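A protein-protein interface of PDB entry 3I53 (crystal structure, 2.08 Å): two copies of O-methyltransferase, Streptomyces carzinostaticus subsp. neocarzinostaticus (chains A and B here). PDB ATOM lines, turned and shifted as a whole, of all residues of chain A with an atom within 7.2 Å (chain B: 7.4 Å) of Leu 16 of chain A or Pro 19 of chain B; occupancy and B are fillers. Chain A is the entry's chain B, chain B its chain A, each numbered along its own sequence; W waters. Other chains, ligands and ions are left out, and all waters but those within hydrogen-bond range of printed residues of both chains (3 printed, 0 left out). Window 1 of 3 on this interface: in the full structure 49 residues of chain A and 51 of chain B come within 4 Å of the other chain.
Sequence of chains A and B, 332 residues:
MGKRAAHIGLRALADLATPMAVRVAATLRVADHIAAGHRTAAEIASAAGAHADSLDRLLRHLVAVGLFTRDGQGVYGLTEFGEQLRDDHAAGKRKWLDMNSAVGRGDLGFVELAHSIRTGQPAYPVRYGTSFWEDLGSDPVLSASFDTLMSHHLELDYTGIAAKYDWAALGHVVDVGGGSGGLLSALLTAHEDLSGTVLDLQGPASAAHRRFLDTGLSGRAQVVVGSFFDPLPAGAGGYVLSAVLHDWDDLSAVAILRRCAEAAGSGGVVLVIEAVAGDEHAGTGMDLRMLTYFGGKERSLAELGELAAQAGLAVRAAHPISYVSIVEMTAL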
ATOM      1  N   ARG A  11     -24.409 -34.040 -28.155  1.00  0.00           N
ATOM      2  CA  ARG A  11     -24.011 -32.695 -27.790  1.00  0.00           C
ATOM      3  C   ARG A  11     -22.802 -32.815 -26.849  1.00  0.00           C
ATOM      4  O   ARG A  11     -21.998 -31.890 -26.721  1.00  0.00           O
ATOM      5  CB  ARG A  11     -25.196 -32.004 -27.115  1.00  0.00           C
ATOM      6  CG  ARG A  11     -25.041 -30.521 -26.853  1.00  0.00           C
ATOM      7  CD  ARG A  11     -26.410 -29.829 -26.913  1.00  0.00           C
ATOM      8  NE  ARG A  11     -26.411 -28.482 -26.341  1.00  0.00           N
ATOM      9  CZ  ARG A  11     -25.486 -27.552 -26.580  1.00  0.00           C
ATOM     10  NH1 ARG A  11     -24.459 -27.809 -27.390  1.00  0.00           N
ATOM     11  NH2 ARG A  11     -25.588 -26.358 -26.009  1.00  0.00           N
ATOM     12  N   ALA A  12     -22.668 -33.983 -26.221  1.00  0.00           N
ATOM     13  CA  ALA A  12     -21.564 -34.257 -25.311  1.00  0.00           C
ATOM     14  C   ALA A  12     -20.305 -34.584 -26.103  1.00  0.00           C
ATOM     15  O   ALA A  12     -19.208 -34.148 -25.753  1.00  0.00           O
ATOM     16  CB  ALA A  12     -21.918 -35.426 -24.399  1.00  0.00           C
ATOM     17  N   LEU A  13     -20.471 -35.372 -27.161  1.00  0.00           N
ATOM     18  CA  LEU A  13     -19.357 -35.754 -28.013  1.00  0.00           C
ATOM     19  C   LEU A  13     -18.739 -34.512 -28.642  1.00  0.00           C
ATOM     20  O   LEU A  13     -17.546 -34.494 -28.955  1.00  0.00           O
ATOM     21  CB  LEU A  13     -19.829 -36.674 -29.141  1.00  0.00           C
ATOM     22  CG  LEU A  13     -19.570 -38.180 -29.117  1.00  0.00           C
ATOM     23  CD1 LEU A  13     -20.119 -38.762 -30.418  1.00  0.00           C
ATOM     24  CD2 LEU A  13     -18.081 -38.491 -28.991  1.00  0.00           C
ATOM     25  N   ALA A  14     -19.560 -33.480 -28.830  1.00  0.00           N
ATOM     26  CA  ALA A  14     -19.099 -32.247 -29.449  1.00  0.00           C
ATOM     27  C   ALA A  14     -18.634 -31.180 -28.473  1.00  0.00           C
ATOM     28  O   ALA A  14     -18.272 -30.079 -28.883  1.00  0.00           O
ATOM     29  CB  ALA A  14     -20.187 -31.677 -30.334  1.00  0.00           C
ATOM     30  N   ASP A  15     -18.614 -31.492 -27.187  1.00  0.00           N
ATOM     31  CA  ASP A  15     -18.202 -30.481 -26.227  1.00  0.00           C
ATOM     32  C   ASP A  15     -16.774 -29.979 -26.425  1.00  0.00           C
ATOM     33  O   ASP A  15     -15.839 -30.758 -26.624  1.00  0.00           O
ATOM     34  CB  ASP A  15     -18.360 -30.985 -24.799  1.00  0.00           C
ATOM     35  CG  ASP A  15     -17.866 -29.976 -23.794  1.00  0.00           C
ATOM     36  OD1 ASP A  15     -18.399 -28.850 -23.801  1.00  0.00           O
ATOM     37  OD2 ASP A  15     -16.945 -30.287 -23.014  1.00  0.00           O
ATOM     38  N   LEU A  16     -16.612 -28.662 -26.359  1.00  0.00           N
ATOM     39  CA  LEU A  16     -15.297 -28.046 -26.535  1.00  0.00           C
ATOM     40  C   LEU A  16     -14.806 -27.453 -25.216  1.00  0.00           C
ATOM     41  O   LEU A  16     -13.609 -27.225 -25.037  1.00  0.00           O
ATOM     42  CB  LEU A  16     -15.369 -26.939 -27.604  1.00  0.00           C
ATOM     43  CG  LEU A  16     -15.661 -27.395 -29.037  1.00  0.00           C
ATOM     44  CD1 LEU A  16     -15.792 -26.192 -29.965  1.00  0.00           C
ATOM     45  CD2 LEU A  16     -14.523 -28.293 -29.504  1.00  0.00           C
ATOM     46  N   ALA A  17     -15.740 -27.212 -24.301  1.00  0.00           N
ATOM     47  CA  ALA A  17     -15.433 -26.625 -22.999  1.00  0.00           C
ATOM     48  C   ALA A  17     -14.398 -27.404 -22.200  1.00  0.00           C
ATOM     49  O   ALA A  17     -13.399 -26.845 -21.742  1.00  0.00           O
ATOM     50  CB  ALA A  17     -16.708 -26.482 -22.172  1.00  0.00           C
ATOM     51  N   THR A  18     -14.628 -28.695 -22.029  1.00  0.00           N
ATOM     52  CA  THR A  18     -13.691 -29.481 -21.255  1.00  0.00           C
ATOM     53  C   THR A  18     -12.314 -29.637 -21.904  1.00  0.00           C
ATOM     54  O   THR A  18     -11.299 -29.454 -21.242  1.00  0.00           O
ATOM     55  CB  THR A  18     -14.300 -30.854 -20.904  1.00  0.00           C
ATOM     56  OG1 THR A  18     -15.397 -30.652 -19.997  1.00  0.00           O
ATOM     57  CG2 THR A  18     -13.259 -31.756 -20.239  1.00  0.00           C
ATOM     58  N   PRO A  19     -12.256 -29.953 -23.204  1.00  0.00           N
ATOM     59  CA  PRO A  19     -10.953 -30.113 -23.867  1.00  0.00           C
ATOM     60  C   PRO A  19     -10.080 -28.850 -23.780  1.00  0.00           C
ATOM     61  O   PRO A  19      -8.874 -28.931 -23.559  1.00  0.00           O
ATOM     62  CB  PRO A  19     -11.335 -30.445 -25.310  1.00  0.00           C
ATOM     63  CG  PRO A  19     -12.701 -31.067 -25.183  1.00  0.00           C
ATOM     64  CD  PRO A  19     -13.366 -30.220 -24.136  1.00  0.00           C
ATOM     65  N   MET A  20     -10.696 -27.687 -23.971  1.00  0.00           N
ATOM     66  CA  MET A  20      -9.974 -26.427 -23.906  1.00  0.00           C
ATOM     67  C   MET A  20      -9.622 -26.098 -22.460  1.00  0.00           C
ATOM     68  O   MET A  20      -8.551 -25.555 -22.196  1.00  0.00           O
ATOM     69  CB  MET A  20     -10.801 -25.290 -24.528  1.00  0.00           C
ATOM     70  CG  MET A  20     -10.962 -25.400 -26.046  1.00  0.00           C
ATOM     71  SD  MET A  20      -9.369 -25.553 -26.922  1.00  0.00           S
ATOM     72  CE  MET A  20      -8.370 -24.318 -26.082  1.00  0.00           C
ATOM     73  N   ALA A  21     -10.515 -26.428 -21.528  1.00  0.00           N
ATOM     74  CA  ALA A  21     -10.245 -26.176 -20.113  1.00  0.00           C
ATOM     75  C   ALA A  21      -8.983 -26.958 -19.742  1.00  0.00           C
ATOM     76  O   ALA A  21      -8.101 -26.436 -19.066  1.00  0.00           O
ATOM     77  CB  ALA A  21     -11.437 -26.627 -19.248  1.00  0.00           C
ATOM     78  N   VAL A  22      -8.892 -28.203 -20.205  1.00  0.00           N
ATOM     79  CA  VAL A  22      -7.730 -29.040 -19.934  1.00  0.00           C
ATOM     80  C   VAL A  22      -6.475 -28.393 -20.516  1.00  0.00           C
ATOM     81  O   VAL A  22      -5.452 -28.251 -19.841  1.00  0.00           O
ATOM     82  CB  VAL A  22      -7.871 -30.438 -20.572  1.00  0.00           C
ATOM     83  CG1 VAL A  22      -6.661 -31.284 -20.235  1.00  0.00           C
ATOM     84  CG2 VAL A  22      -9.142 -31.114 -20.100  1.00  0.00           C
ATOM     85  N   VAL A 111      -9.915 -26.175 -34.862  1.00  0.00           N
ATOM     86  CA  VAL A 111     -11.072 -25.293 -34.867  1.00  0.00           C
ATOM     87  C   VAL A 111     -11.411 -24.831 -36.288  1.00  0.00           C
ATOM     88  O   VAL A 111     -12.534 -24.382 -36.536  1.00  0.00           O
ATOM     89  CB  VAL A 111     -10.869 -24.053 -33.938  1.00  0.00           C
ATOM     90  CG1 VAL A 111      -9.966 -23.003 -34.617  1.00  0.00           C
ATOM     91  CG2 VAL A 111     -12.226 -23.446 -33.573  1.00  0.00           C
ATOM     92  N   LEU A 113     -11.118 -26.948 -38.942  1.00  0.00           N
ATOM     93  CA  LEU A 113     -11.285 -28.187 -39.690  1.00  0.00           C
ATOM     94  C   LEU A 113     -12.205 -28.093 -40.913  1.00  0.00           C
ATOM     95  O   LEU A 113     -12.001 -28.789 -41.910  1.00  0.00           O
ATOM     96  CB  LEU A 113     -11.793 -29.289 -38.747  1.00  0.00           C
ATOM     97  CG  LEU A 113     -12.032 -30.688 -39.335  1.00  0.00           C
ATOM     98  CD1 LEU A 113     -10.720 -31.284 -39.804  1.00  0.00           C
ATOM     99  CD2 LEU A 113     -12.673 -31.579 -38.286  1.00  0.00           C
ATOM    100  N   ALA B  12      -7.490 -38.072 -24.212  1.00  0.00           N
ATOM    101  CA  ALA B  12      -8.822 -38.254 -24.769  1.00  0.00           C
ATOM    102  C   ALA B  12      -9.771 -37.166 -24.283  1.00  0.00           C
ATOM    103  O   ALA B  12     -10.685 -36.744 -24.998  1.00  0.00           O
ATOM    104  CB  ALA B  12      -9.359 -39.628 -24.392  1.00  0.00           C
ATOM    105  N   LEU B  13      -9.540 -36.721 -23.054  1.00  0.00           N
ATOM    106  CA  LEU B  13     -10.354 -35.693 -22.429  1.00  0.00           C
ATOM    107  C   LEU B  13     -10.061 -34.343 -23.066  1.00  0.00           C
ATOM    108  O   LEU B  13     -10.884 -33.434 -23.023  1.00  0.00           O
ATOM    109  CB  LEU B  13     -10.026 -35.636 -20.942  1.00  0.00           C
ATOM    110  CG  LEU B  13     -11.149 -35.302 -19.970  1.00  0.00           C
ATOM    111  CD1 LEU B  13     -12.316 -36.265 -20.155  1.00  0.00           C
ATOM    112  CD2 LEU B  13     -10.594 -35.391 -18.556  1.00  0.00           C
ATOM    113  N   ALA B  14      -8.877 -34.219 -23.653  1.00  0.00           N
ATOM    114  CA  ALA B  14      -8.467 -32.974 -24.288  1.00  0.00           C
ATOM    115  C   ALA B  14      -8.644 -33.030 -25.806  1.00  0.00           C
ATOM    116  O   ALA B  14      -8.335 -32.066 -26.515  1.00  0.00           O
ATOM    117  CB  ALA B  14      -7.003 -32.680 -23.945  1.00  0.00           C
ATOM    118  N   ASP B  15      -9.139 -34.157 -26.308  1.00  0.00           N
ATOM    119  CA  ASP B  15      -9.309 -34.298 -27.738  1.00  0.00           C
ATOM    120  C   ASP B  15     -10.197 -33.231 -28.362  1.00  0.00           C
ATOM    121  O   ASP B  15     -11.262 -32.911 -27.840  1.00  0.00           O
ATOM    122  CB  ASP B  15      -9.875 -35.669 -28.096  1.00  0.00           C
ATOM    123  CG  ASP B  15      -9.836 -35.921 -29.585  1.00  0.00           C
ATOM    124  OD1 ASP B  15      -8.732 -35.790 -30.152  1.00  0.00           O
ATOM    125  OD2 ASP B  15     -10.887 -36.233 -30.186  1.00  0.00           O
ATOM    126  N   LEU B  16      -9.738 -32.693 -29.489  1.00  0.00           N
ATOM    127  CA  LEU B  16     -10.467 -31.669 -30.230  1.00  0.00           C
ATOM    128  C   LEU B  16     -10.923 -32.227 -31.583  1.00  0.00           C
ATOM    129  O   LEU B  16     -11.884 -31.720 -32.174  1.00  0.00           O
ATOM    130  CB  LEU B  16      -9.582 -30.435 -30.447  1.00  0.00           C
ATOM    131  CG  LEU B  16      -9.256 -29.621 -29.194  1.00  0.00           C
ATOM    132  CD1 LEU B  16      -8.235 -28.536 -29.519  1.00  0.00           C
ATOM    133  CD2 LEU B  16     -10.537 -29.016 -28.638  1.00  0.00           C
ATOM    134  N   ALA B  17     -10.239 -33.276 -32.053  1.00  0.00           N
ATOM    135  CA  ALA B  17     -10.553 -33.902 -33.329  1.00  0.00           C
ATOM    136  C   ALA B  17     -12.011 -34.360 -33.458  1.00  0.00           C
ATOM    137  O   ALA B  17     -12.695 -33.986 -34.417  1.00  0.00           O
ATOM    138  CB  ALA B  17      -9.619 -35.085 -33.576  1.00  0.00           C
ATOM    139  N   THR B  18     -12.473 -35.173 -32.506  1.00  0.00           N
ATOM    140  CA  THR B  18     -13.842 -35.677 -32.525  1.00  0.00           C
ATOM    141  C   THR B  18     -14.917 -34.583 -32.382  1.00  0.00           C
ATOM    142  O   THR B  18     -15.872 -34.557 -33.147  1.00  0.00           O
ATOM    143  CB  THR B  18     -14.042 -36.767 -31.437  1.00  0.00           C
ATOM    144  OG1 THR B  18     -13.209 -37.890 -31.745  1.00  0.00           O
ATOM    145  CG2 THR B  18     -15.485 -37.230 -31.382  1.00  0.00           C
ATOM    146  N   PRO B  19     -14.775 -33.669 -31.410  1.00  0.00           N
ATOM    147  CA  PRO B  19     -15.795 -32.615 -31.268  1.00  0.00           C
ATOM    148  C   PRO B  19     -15.931 -31.771 -32.535  1.00  0.00           C
ATOM    149  O   PRO B  19     -17.038 -31.408 -32.933  1.00  0.00           O
ATOM    150  CB  PRO B  19     -15.288 -31.768 -30.099  1.00  0.00           C
ATOM    151  CG  PRO B  19     -14.426 -32.700 -29.328  1.00  0.00           C
ATOM    152  CD  PRO B  19     -13.738 -33.550 -30.370  1.00  0.00           C
ATOM    153  N   MET B  20     -14.804 -31.437 -33.155  1.00  0.00           N
ATOM    154  CA  MET B  20     -14.846 -30.629 -34.369  1.00  0.00           C
ATOM    155  C   MET B  20     -15.344 -31.453 -35.550  1.00  0.00           C
ATOM    156  O   MET B  20     -16.043 -30.927 -36.417  1.00  0.00           O
ATOM    157  CB  MET B  20     -13.470 -30.008 -34.680  1.00  0.00           C
ATOM    158  CG  MET B  20     -13.048 -28.898 -33.704  1.00  0.00           C
ATOM    159  SD  MET B  20     -14.242 -27.538 -33.581  1.00  0.00           S
ATOM    160  CE  MET B  20     -14.377 -27.074 -35.351  1.00  0.00           C
ATOM    161  N   ALA B  21     -15.011 -32.745 -35.580  1.00  0.00           N
ATOM    162  CA  ALA B  21     -15.468 -33.609 -36.670  1.00  0.00           C
ATOM    163  C   ALA B  21     -16.984 -33.655 -36.657  1.00  0.00           C
ATOM    164  O   ALA B  21     -17.633 -33.561 -37.699  1.00  0.00           O
ATOM    165  CB  ALA B  21     -14.903 -35.015 -36.511  1.00  0.00           C
ATOM    166  N   VAL B  22     -17.542 -33.814 -35.465  1.00  0.00           N
ATOM    167  CA  VAL B  22     -18.982 -33.855 -35.294  1.00  0.00           C
ATOM    168  C   VAL B  22     -19.609 -32.524 -35.739  1.00  0.00           C
ATOM    169  O   VAL B  22     -20.625 -32.509 -36.442  1.00  0.00           O
ATOM    170  CB  VAL B  22     -19.369 -34.112 -33.813  1.00  0.00           C
ATOM    171  CG1 VAL B  22     -20.884 -34.060 -33.666  1.00  0.00           C
ATOM    172  CG2 VAL B  22     -18.837 -35.488 -33.351  1.00  0.00           C
ATOM    173  N   ARG B  23     -18.999 -31.418 -35.320  1.00  0.00           N
ATOM    174  CA  ARG B  23     -19.494 -30.099 -35.678  1.00  0.00           C
ATOM    175  C   ARG B  23     -19.390 -29.830 -37.177  1.00  0.00           C
ATOM    176  O   ARG B  23     -20.255 -29.170 -37.743  1.00  0.00           O
ATOM    177  CB  ARG B  23     -18.759 -29.016 -34.876  1.00  0.00           C
ATOM    178  CG  ARG B  23     -19.206 -28.951 -33.420  1.00  0.00           C
ATOM    179  CD  ARG B  23     -18.217 -28.196 -32.533  1.00  0.00           C
ATOM    180  NE  ARG B  23     -18.631 -28.237 -31.134  1.00  0.00           N
ATOM    181  CZ  ARG B  23     -19.645 -27.541 -30.619  1.00  0.00           C
ATOM    182  NH1 ARG B  23     -20.357 -26.729 -31.384  1.00  0.00           N
ATOM    183  NH2 ARG B  23     -19.961 -27.680 -29.339  1.00  0.00           N
ATOM    184  N   VAL B  24     -18.350 -30.336 -37.826  1.00  0.00           N
ATOM    185  CA  VAL B  24     -18.227 -30.130 -39.266  1.00  0.00           C
ATOM    186  C   VAL B  24     -19.321 -30.937 -39.975  1.00  0.00           C
ATOM    187  O   VAL B  24     -20.017 -30.418 -40.844  1.00  0.00           O
ATOM    188  CB  VAL B  24     -16.845 -30.562 -39.802  1.00  0.00           C
ATOM    189  CG1 VAL B  24     -16.845 -30.538 -41.338  1.00  0.00           C
ATOM    190  CG2 VAL B  24     -15.770 -29.613 -39.281  1.00  0.00           C
ATOM    191  N   ALA B  25     -19.486 -32.200 -39.592  1.00  0.00           N
ATOM    192  CA  ALA B  25     -20.517 -33.027 -40.208  1.00  0.00           C
ATOM    193  C   ALA B  25     -21.895 -32.412 -39.988  1.00  0.00           C
ATOM    194  O   ALA B  25     -22.727 -32.398 -40.900  1.00  0.00           O
ATOM    195  CB  ALA B  25     -20.486 -34.438 -39.636  1.00  0.00           C
ATOM    196  N   HIS B  61     -13.452 -41.247 -39.501  1.00  0.00           N
ATOM    197  CA  HIS B  61     -13.349 -40.911 -38.089  1.00  0.00           C
ATOM    198  C   HIS B  61     -14.702 -41.012 -37.421  1.00  0.00           C
ATOM    199  O   HIS B  61     -14.807 -41.528 -36.311  1.00  0.00           O
ATOM    200  CB  HIS B  61     -12.819 -39.486 -37.882  1.00  0.00           C
ATOM    201  CG  HIS B  61     -12.567 -39.144 -36.442  1.00  0.00           C
ATOM    202  ND1 HIS B  61     -11.487 -39.637 -35.737  1.00  0.00           N
ATOM    203  CD2 HIS B  61     -13.290 -38.415 -35.557  1.00  0.00           C
ATOM    204  CE1 HIS B  61     -11.561 -39.231 -34.481  1.00  0.00           C
ATOM    205  NE2 HIS B  61     -12.647 -38.489 -34.344  1.00  0.00           N
ATOM    206  N   LEU B  62     -15.745 -40.511 -38.081  1.00  0.00           N
ATOM    207  CA  LEU B  62     -17.073 -40.565 -37.474  1.00  0.00           C
ATOM    208  C   LEU B  62     -17.649 -41.973 -37.447  1.00  0.00           C
ATOM    209  O   LEU B  62     -18.528 -42.271 -36.635  1.00  0.00           O
ATOM    210  CB  LEU B  62     -18.033 -39.585 -38.159  1.00  0.00           C
ATOM    211  CG  LEU B  62     -17.641 -38.126 -37.885  1.00  0.00           C
ATOM    212  CD1 LEU B  62     -18.682 -37.186 -38.444  1.00  0.00           C
ATOM    213  CD2 LEU B  62     -17.492 -37.913 -36.390  1.00  0.00           C
ATOM    214  N   VAL B  65     -16.349 -43.422 -34.446  1.00  0.00           N
ATOM    215  CA  VAL B  65     -17.060 -42.913 -33.286  1.00  0.00           C
ATOM    216  C   VAL B  65     -18.437 -43.558 -33.176  1.00  0.00           C
ATOM    217  O   VAL B  65     -19.103 -43.449 -32.150  1.00  0.00           O
ATOM    218  CB  VAL B  65     -17.173 -41.365 -33.352  1.00  0.00           C
ATOM    219  CG1 VAL B  65     -18.180 -40.840 -32.332  1.00  0.00           C
ATOM    220  CG2 VAL B  65     -15.798 -40.761 -33.089  1.00  0.00           C
ATOM    221  N   LEU B  97     -25.125 -27.648 -33.055  1.00  0.00           N
ATOM    222  CA  LEU B  97     -23.772 -27.931 -33.525  1.00  0.00           C
ATOM    223  C   LEU B  97     -23.367 -27.242 -34.815  1.00  0.00           C
ATOM    224  O   LEU B  97     -22.177 -27.056 -35.073  1.00  0.00           O
ATOM    225  CB  LEU B  97     -23.595 -29.438 -33.694  1.00  0.00           C
ATOM    226  CG  LEU B  97     -23.174 -30.227 -32.454  1.00  0.00           C
ATOM    227  CD1 LEU B  97     -24.004 -29.829 -31.236  1.00  0.00           C
ATOM    228  CD2 LEU B  97     -23.318 -31.706 -32.764  1.00  0.00           C
ATOM    229  N   GLY B 104     -23.611 -22.662 -32.296  1.00  0.00           N
ATOM    230  CA  GLY B 104     -22.630 -23.448 -33.015  1.00  0.00           C
ATOM    231  C   GLY B 104     -21.454 -22.552 -33.362  1.00  0.00           C
ATOM    232  O   GLY B 104     -20.280 -22.951 -33.296  1.00  0.00           O
ATOM    233  N   GLY B 106     -20.789 -19.636 -31.752  1.00  0.00           N
ATOM    234  CA  GLY B 106     -20.216 -19.199 -30.481  1.00  0.00           C
ATOM    235  C   GLY B 106     -19.328 -20.182 -29.742  1.00  0.00           C
ATOM    236  O   GLY B 106     -18.341 -19.782 -29.139  1.00  0.00           O
ATOM    237  N   ASP B 107     -19.669 -21.466 -29.770  1.00  0.00           N
ATOM    238  CA  ASP B 107     -18.849 -22.452 -29.077  1.00  0.00           C
ATOM    239  C   ASP B 107     -17.434 -22.570 -29.630  1.00  0.00           C
ATOM    240  O   ASP B 107     -16.548 -23.061 -28.937  1.00  0.00           O
ATOM    241  CB  ASP B 107     -19.513 -23.830 -29.082  1.00  0.00           C
ATOM    242  CG  ASP B 107     -20.607 -23.953 -28.039  1.00  0.00           C
ATOM    243  OD1 ASP B 107     -21.166 -25.062 -27.915  1.00  0.00           O
ATOM    244  OD2 ASP B 107     -20.916 -22.950 -27.351  1.00  0.00           O
ATOM    245  N   LEU B 108     -17.207 -22.140 -30.867  1.00  0.00           N
ATOM    246  CA  LEU B 108     -15.858 -22.214 -31.418  1.00  0.00           C
ATOM    247  C   LEU B 108     -14.961 -21.226 -30.672  1.00  0.00           C
ATOM    248  O   LEU B 108     -13.730 -21.340 -30.700  1.00  0.00           O
ATOM    249  CB  LEU B 108     -15.856 -21.915 -32.918  1.00  0.00           C
ATOM    250  CG  LEU B 108     -16.629 -22.895 -33.807  1.00  0.00           C
ATOM    251  CD1 LEU B 108     -16.223 -22.659 -35.263  1.00  0.00           C
ATOM    252  CD2 LEU B 108     -16.320 -24.352 -33.418  1.00  0.00           C
ATOM    253  N   GLY B 109     -15.597 -20.267 -30.000  1.00  0.00           N
ATOM    254  CA  GLY B 109     -14.871 -19.277 -29.224  1.00  0.00           C
ATOM    255  C   GLY B 109     -14.086 -19.915 -28.089  1.00  0.00           C
ATOM    256  O   GLY B 109     -13.140 -19.322 -27.569  1.00  0.00           O
ATOM    257  N   PHE B 110     -14.473 -21.128 -27.697  1.00  0.00           N
ATOM    258  CA  PHE B 110     -13.754 -21.831 -26.647  1.00  0.00           C
ATOM    259  C   PHE B 110     -12.294 -22.006 -27.057  1.00  0.00           C
ATOM    260  O   PHE B 110     -11.412 -22.189 -26.215  1.00  0.00           O
ATOM    261  CB  PHE B 110     -14.382 -23.205 -26.380  1.00  0.00           C
ATOM    262  CG  PHE B 110     -15.504 -23.175 -25.377  1.00  0.00           C
ATOM    263  CD1 PHE B 110     -16.794 -23.529 -25.745  1.00  0.00           C
ATOM    264  CD2 PHE B 110     -15.265 -22.785 -24.068  1.00  0.00           C
ATOM    265  CE1 PHE B 110     -17.840 -23.492 -24.822  1.00  0.00           C
ATOM    266  CE2 PHE B 110     -16.300 -22.743 -23.127  1.00  0.00           C
ATOM    267  CZ  PHE B 110     -17.587 -23.095 -23.505  1.00  0.00           C
ATOM    268  N   VAL B 111     -12.019 -21.950 -28.353  1.00  0.00           N
ATOM    269  CA  VAL B 111     -10.635 -22.106 -28.775  1.00  0.00           C
ATOM    270  C   VAL B 111      -9.771 -20.981 -28.184  1.00  0.00           C
ATOM    271  O   VAL B 111      -8.559 -21.145 -28.032  1.00  0.00           O
ATOM    272  CB  VAL B 111     -10.500 -22.102 -30.327  1.00  0.00           C
ATOM    273  CG1 VAL B 111     -10.599 -20.670 -30.866  1.00  0.00           C
ATOM    274  CG2 VAL B 111      -9.205 -22.794 -30.743  1.00  0.00           C
ATOM    275  N   LEU B 113     -10.191 -19.682 -25.112  1.00  0.00           N
ATOM    276  CA  LEU B 113     -10.416 -19.702 -23.664  1.00  0.00           C
ATOM    277  C   LEU B 113      -9.253 -19.172 -22.816  1.00  0.00           C
ATOM    278  O   LEU B 113      -9.467 -18.614 -21.739  1.00  0.00           O
ATOM    279  CB  LEU B 113     -10.753 -21.127 -23.218  1.00  0.00           C
ATOM    280  CG  LEU B 113     -11.035 -21.362 -21.725  1.00  0.00           C
ATOM    281  CD1 LEU B 113     -12.261 -20.578 -21.289  1.00  0.00           C
ATOM    282  CD2 LEU B 113     -11.245 -22.846 -21.488  1.00  0.00           C
ATOM    283  N   ARG B 289     -19.172 -21.294 -20.560  1.00  0.00           N
ATOM    284  CA  ARG B 289     -19.765 -20.820 -21.805  1.00  0.00           C
ATOM    285  C   ARG B 289     -20.107 -19.340 -21.652  1.00  0.00           C
ATOM    286  O   ARG B 289     -19.834 -18.533 -22.544  1.00  0.00           O
ATOM    287  CB  ARG B 289     -21.036 -21.612 -22.169  1.00  0.00           C
ATOM    288  CG  ARG B 289     -21.701 -21.096 -23.474  1.00  0.00           C
ATOM    289  CD  ARG B 289     -22.840 -21.975 -24.030  1.00  0.00           C
ATOM    290  NE  ARG B 289     -22.369 -23.178 -24.720  1.00  0.00           N
ATOM    291  CZ  ARG B 289     -22.100 -24.333 -24.116  1.00  0.00           C
ATOM    292  NH1 ARG B 289     -22.254 -24.458 -22.797  1.00  0.00           N
ATOM    293  NH2 ARG B 289     -21.684 -25.376 -24.826  1.00  0.00           N
HETATM  294  O   HOH W   1     -21.150 -28.416 -24.463  1.00  0.00           O
HETATM  295  O   HOH W   2     -21.605 -29.311 -27.106  1.00  0.00           O
HETATM  296  O   HOH W   3     -18.902 -26.953 -26.334  1.00  0.00           O
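The backbone NH (N) of Ala 17 of chain A lies within hydrogen-bond range of the side-chain carboxylate (OD1) of Asp 15 of chain A, at 3.2 Å.
The side-chain carboxylate of Asp 107 of chain B is in salt-bridge range of the guanidinium group of Arg 289 of chain B (3.0 Å).
The side-chain hydroxyl of Thr 18 of chain B sits at hydrogen-bond distance from a ring nitrogen (NE2) of His 61 of chain B (2.7 Å).
O of Leu 13 of chain A touches CA of Pro 19 of chain B (3.5 Å).
Leu 13 of chain A touches Val 65 of chain B (CD1 to CG1, 3.4 Å).
O of Asp 15 of chain A touches CG of Pro 19 of chain B (3.6 Å).
Pro 19 of chain B touches Leu 16 of chain A.
Asp 107 of chain B touches Leu 16 of chain A (O to CD1, 3.4 Å).
CZ of Phe 110 of chain B touches CB of Ala 17 of chain A, at 3.7 Å.
O of Leu 13 of chain B touches CA of Pro 19 of chain A, 3.4 Å away.
Leu 113 of chain B touches Ala 21 of chain A (CD2 to N, 3.7 Å).
Water W2 bridges O of Arg 11 of chain A (2.6 Å) and NH2 of Arg 23 of chain B (3.2 Å).
Water W3 lies within hydrogen-bond range of the backbone NH (N) of Leu 16 of chain A (2.9 Å), the side-chain carboxylate (OD1) of Asp 15 of chain A (3.2 Å), the guanidinium group (NH2) of Arg 23 of chain B (3.3 Å) and the side-chain carboxylate (OD1) of Asp 107 of chain B (3.3 Å).
Water W1 bridges OD1 of Asp 15 of chain A (2.9 Å) and NH2 of Arg 289 of chain B (3.1 Å).
Leu 13 of chain A touches Thr 18 of chain B, but with the chains exchanged Thr 18 of chain A does not touch Leu 13 of chain B (4.03 Å).
Leu 13 of chain A touches Pro 19 of chain B, and with the chains exchanged Pro 19 of chain A touches Leu 13 of chain B.
Met 20 of chain A touches Val 111 of chain B, and with the chains exchanged Val 111 of chain A touches Met 20 of chain B.
Val 111 of chain B touches its own counterpart, Val 111 of chain A.
Positions printed for both chains: 12, 13, 14, 15, 16, 17, 18, 19, 20, 21, 22, 111 and 113.
The guanidinium group (NE) of Arg 23 of chain B is in hydrogen-bond range of the backbone carbonyl oxygen (O) of Ala 14 of chain A, 2.9 Å away.
Ala 12 of chain A touches none of the printed residues of chain B.
Leu 16 of chain A touches just these residues of chain B: Pro 19, Arg 23, Asp 107 and Leu 108.
Of the printed residues of chain B, Leu 113 of chain A touches Met 20 (3.8 Å), Ala 21 (3.8 Å) and Val 24 (3.8 Å).
Printed residues of chain A within 4 Å of Asp 15 of chain B: Pro 19 (3.5 Å).
Printed residues of chain A within 4 Å of Thr 18 of chain B: Leu 13.
Pro 19 of chain B touches just these residues of chain A: Leu 13, Ala 14, Asp 15 and Leu 16.
Of the printed residues of chain A, Met 20 of chain B touches Val 111 and Leu 113.
Of the 14 printed residues of chain A, 11 touch a printed residue of chain B.
Printed residues of chain A that touch a printed residue of chain B: Leu 13, Ala 14, Asp 15, Leu 16, Ala 17, Pro 19, Met 20, Ala 21, Val 22, Val 111 and Leu 113.
Hydrophobic or aromatic side chains of chain A within 4 Å of the printed part of chain B: Leu 13, Ala 14, Leu 16, Ala 17, Pro 19, Met 20, Val 22, Val 111 and Leu 113.
Of the 27 printed residues of chain B, 17 touch a printed residue of chain A.
Among the printed residues, 27 pairs touch across the chains.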
